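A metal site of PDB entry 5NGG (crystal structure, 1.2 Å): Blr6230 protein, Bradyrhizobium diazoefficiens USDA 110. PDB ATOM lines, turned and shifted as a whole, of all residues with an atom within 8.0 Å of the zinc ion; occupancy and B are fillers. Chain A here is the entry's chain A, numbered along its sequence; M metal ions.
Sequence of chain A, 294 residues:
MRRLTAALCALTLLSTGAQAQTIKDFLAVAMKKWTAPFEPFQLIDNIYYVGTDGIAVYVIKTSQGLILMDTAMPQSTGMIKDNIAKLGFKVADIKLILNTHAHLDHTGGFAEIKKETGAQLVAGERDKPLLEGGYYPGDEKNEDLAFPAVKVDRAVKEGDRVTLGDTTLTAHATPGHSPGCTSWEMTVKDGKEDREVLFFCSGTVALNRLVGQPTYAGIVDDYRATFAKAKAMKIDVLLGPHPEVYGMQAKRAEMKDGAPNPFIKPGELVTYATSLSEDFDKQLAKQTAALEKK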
ATOM      1  N   LYS A 157       9.172 -24.189  14.392  1.00  0.00           N
ATOM      2  CA  LYS A 157       9.081 -24.666  15.771  1.00  0.00           C
ATOM      3  C   LYS A 157      10.252 -25.608  16.053  1.00  0.00           C
ATOM      4  O   LYS A 157      11.061 -25.918  15.164  1.00  0.00           O
ATOM      5  CB  LYS A 157       7.748 -25.348  16.015  1.00  0.00           C
ATOM      6  CG  LYS A 157       6.571 -24.385  15.964  1.00  0.00           C
ATOM      7  CD  LYS A 157       5.302 -25.017  16.509  1.00  0.00           C
ATOM      8  N   GLU A 158      10.347 -26.057  17.300  1.00  0.00           N
ATOM      9  CA  GLU A 158      11.412 -26.952  17.752  1.00  0.00           C
ATOM     10  C   GLU A 158      11.641 -28.104  16.778  1.00  0.00           C
ATOM     11  O   GLU A 158      10.708 -28.854  16.448  1.00  0.00           O
ATOM     12  CB  GLU A 158      11.074 -27.491  19.134  1.00  0.00           C
ATOM     13  CG  GLU A 158      12.004 -28.574  19.692  1.00  0.00           C
ATOM     14  CD  GLU A 158      13.393 -28.099  20.053  1.00  0.00           C
ATOM     15  OE1 GLU A 158      13.610 -26.889  20.291  1.00  0.00           O
ATOM     16  OE2 GLU A 158      14.299 -28.975  20.115  1.00  0.00           O
ATOM     17  N   GLY A 159      12.889 -28.259  16.356  1.00  0.00           N
ATOM     18  CA  GLY A 159      13.322 -29.363  15.514  1.00  0.00           C
ATOM     19  C   GLY A 159      13.223 -29.154  14.020  1.00  0.00           C
ATOM     20  O   GLY A 159      13.700 -29.992  13.258  1.00  0.00           O
ATOM     21  N   THR A 170      19.115 -26.335  12.169  1.00  0.00           N
ATOM     22  CA  THR A 170      18.000 -26.874  12.942  1.00  0.00           C
ATOM     23  C   THR A 170      17.534 -25.807  13.947  1.00  0.00           C
ATOM     24  O   THR A 170      18.348 -25.237  14.692  1.00  0.00           O
ATOM     25  CB  THR A 170      18.405 -28.143  13.685  1.00  0.00           C
ATOM     26  OG1 THR A 170      18.831 -29.113  12.726  1.00  0.00           O
ATOM     27  CG2 THR A 170      17.245 -28.729  14.482  1.00  0.00           C
ATOM     28  N   ALA A 171      16.229 -25.528  13.956  1.00  0.00           N
ATOM     29  CA  ALA A 171      15.618 -24.603  14.900  1.00  0.00           C
ATOM     30  C   ALA A 171      15.450 -25.231  16.257  1.00  0.00           C
ATOM     31  O   ALA A 171      14.931 -26.357  16.365  1.00  0.00           O
ATOM     32  CB  ALA A 171      14.263 -24.146  14.362  1.00  0.00           C
ATOM     33  N   HIS A 172      15.791 -24.483  17.296  1.00  0.00           N
ATOM     34  CA  HIS A 172      15.448 -24.838  18.672  1.00  0.00           C
ATOM     35  C   HIS A 172      14.633 -23.735  19.301  1.00  0.00           C
ATOM     36  O   HIS A 172      15.024 -22.571  19.275  1.00  0.00           O
ATOM     37  CB  HIS A 172      16.699 -25.068  19.501  1.00  0.00           C
ATOM     38  CG  HIS A 172      17.506 -26.225  19.069  1.00  0.00           C
ATOM     39  ND1 HIS A 172      17.278 -27.510  19.509  1.00  0.00           N
ATOM     40  CD2 HIS A 172      18.531 -26.294  18.190  1.00  0.00           C
ATOM     41  CE1 HIS A 172      18.143 -28.319  18.939  1.00  0.00           C
ATOM     42  NE2 HIS A 172      18.918 -27.608  18.147  1.00  0.00           N
ATOM     43  N   ALA A 173      13.507 -24.093  19.924  1.00  0.00           N
ATOM     44  CA  ALA A 173      12.661 -23.100  20.583  1.00  0.00           C
ATOM     45  C   ALA A 173      13.254 -22.783  21.939  1.00  0.00           C
ATOM     46  O   ALA A 173      13.322 -23.644  22.816  1.00  0.00           O
ATOM     47  CB  ALA A 173      11.243 -23.628  20.713  1.00  0.00           C
ATOM     48  N   THR A 174      13.726 -21.550  22.091  1.00  0.00           N
ATOM     49  CA  THR A 174      14.373 -21.086  23.304  1.00  0.00           C
ATOM     50  C   THR A 174      13.731 -19.752  23.720  1.00  0.00           C
ATOM     51  O   THR A 174      14.415 -18.723  23.825  1.00  0.00           O
ATOM     52  CB  THR A 174      15.893 -20.937  23.112  1.00  0.00           C
ATOM     53  OG1 THR A 174      16.158 -20.216  21.902  1.00  0.00           O
ATOM     54  CG2 THR A 174      16.571 -22.279  22.991  1.00  0.00           C
ATOM     55  N   SER A 183      16.970 -20.452  18.639  1.00  0.00           N
ATOM     56  CA  SER A 183      18.396 -20.722  18.552  1.00  0.00           C
ATOM     57  C   SER A 183      18.650 -21.716  17.429  1.00  0.00           C
ATOM     58  O   SER A 183      17.957 -22.706  17.321  1.00  0.00           O
ATOM     59  CB  SER A 183      18.913 -21.266  19.880  1.00  0.00           C
ATOM     60  OG  SER A 183      18.744 -20.292  20.925  1.00  0.00           O
ATOM     61  N   GLU A 185      21.000 -24.327  15.209  1.00  0.00           N
ATOM     62  CA  GLU A 185      22.142 -25.233  15.284  1.00  0.00           C
ATOM     63  C   GLU A 185      22.613 -25.638  13.890  1.00  0.00           C
ATOM     64  O   GLU A 185      21.802 -25.935  13.003  1.00  0.00           O
ATOM     65  CB  GLU A 185      21.749 -26.479  16.076  1.00  0.00           C
ATOM     66  CG  GLU A 185      22.860 -27.491  16.252  1.00  0.00           C
ATOM     67  CD  GLU A 185      22.431 -28.709  17.052  1.00  0.00           C
ATOM     68  OE1 GLU A 185      21.226 -28.847  17.418  1.00  0.00           O
ATOM     69  OE2 GLU A 185      23.333 -29.559  17.291  1.00  0.00           O
ATOM     70  N   LEU A 198      25.918 -23.227  17.816  1.00  0.00           N
ATOM     71  CA  LEU A 198      24.602 -22.685  18.145  1.00  0.00           C
ATOM     72  C   LEU A 198      24.636 -21.194  18.017  1.00  0.00           C
ATOM     73  O   LEU A 198      25.360 -20.521  18.748  1.00  0.00           O
ATOM     74  CB  LEU A 198      24.142 -23.078  19.544  1.00  0.00           C
ATOM     75  CG  LEU A 198      22.668 -22.811  19.857  1.00  0.00           C
ATOM     76  CD1 LEU A 198      21.768 -23.758  19.089  1.00  0.00           C
ATOM     77  CD2 LEU A 198      22.386 -22.859  21.345  1.00  0.00           C
ATOM     78  N   LYS A 229      17.486 -25.916  29.135  1.00  0.00           N
ATOM     79  CA  LYS A 229      17.696 -26.476  27.798  1.00  0.00           C
ATOM     80  C   LYS A 229      19.105 -26.159  27.303  1.00  0.00           C
ATOM     81  O   LYS A 229      19.825 -27.053  26.829  1.00  0.00           O
ATOM     82  CB  LYS A 229      16.652 -25.929  26.829  1.00  0.00           C
ATOM     83  CG  LYS A 229      16.771 -26.392  25.382  1.00  0.00           C
ATOM     84  CD  LYS A 229      15.627 -25.825  24.554  1.00  0.00           C
ATOM     85  CE  LYS A 229      15.767 -26.097  23.082  1.00  0.00           C
ATOM     86  NZ  LYS A 229      15.707 -27.533  22.795  1.00  0.00           N
ATOM     87  N   MET A 233      22.457 -28.833  26.097  1.00  0.00           N
ATOM     88  CA  MET A 233      22.771 -28.998  24.683  1.00  0.00           C
ATOM     89  C   MET A 233      24.247 -29.231  24.456  1.00  0.00           C
ATOM     90  O   MET A 233      25.071 -28.579  25.046  1.00  0.00           O
ATOM     91  CB  MET A 233      22.350 -27.753  23.909  1.00  0.00           C
ATOM     92  CG  MET A 233      20.846 -27.540  23.834  1.00  0.00           C
ATOM     93  SD  MET A 233      20.311 -26.077  22.966  1.00  0.00           S
ATOM     94  CE  MET A 233      20.933 -26.673  21.412  1.00  0.00           C
HETATM   95 ZN    ZN M   1      15.970 -28.278  20.873  1.00  0.00          ZN
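A ring nitrogen (NE2) of His 172 is in hydrogen-bond range of the side-chain carboxylate (OE1) of Glu 185 (2.7 Å).
The backbone NH (N) of His 172 sits at hydrogen-bond distance from the backbone carbonyl oxygen (O) of Ser 183 (2.8 Å).
The backbone NH (N) of Ala 173 lies within hydrogen-bond range of the side-chain carboxylate (OE1) of Glu 158, at 2.8 Å.
Of the 13 residues printed, 3 come within 4 Å of the zinc ion.
The zinc ion is bound by OE2 of Glu 158 (2.0 Å), ND1 of His 172 (2.0 Å) and NZ of Lys 229 (2.1 Å).
The zinc ion has three donor atoms within binding distance.
Slightly farther from the zinc ion lies the side-chain carboxylate (OE1) of Glu 158 (2.8 Å).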
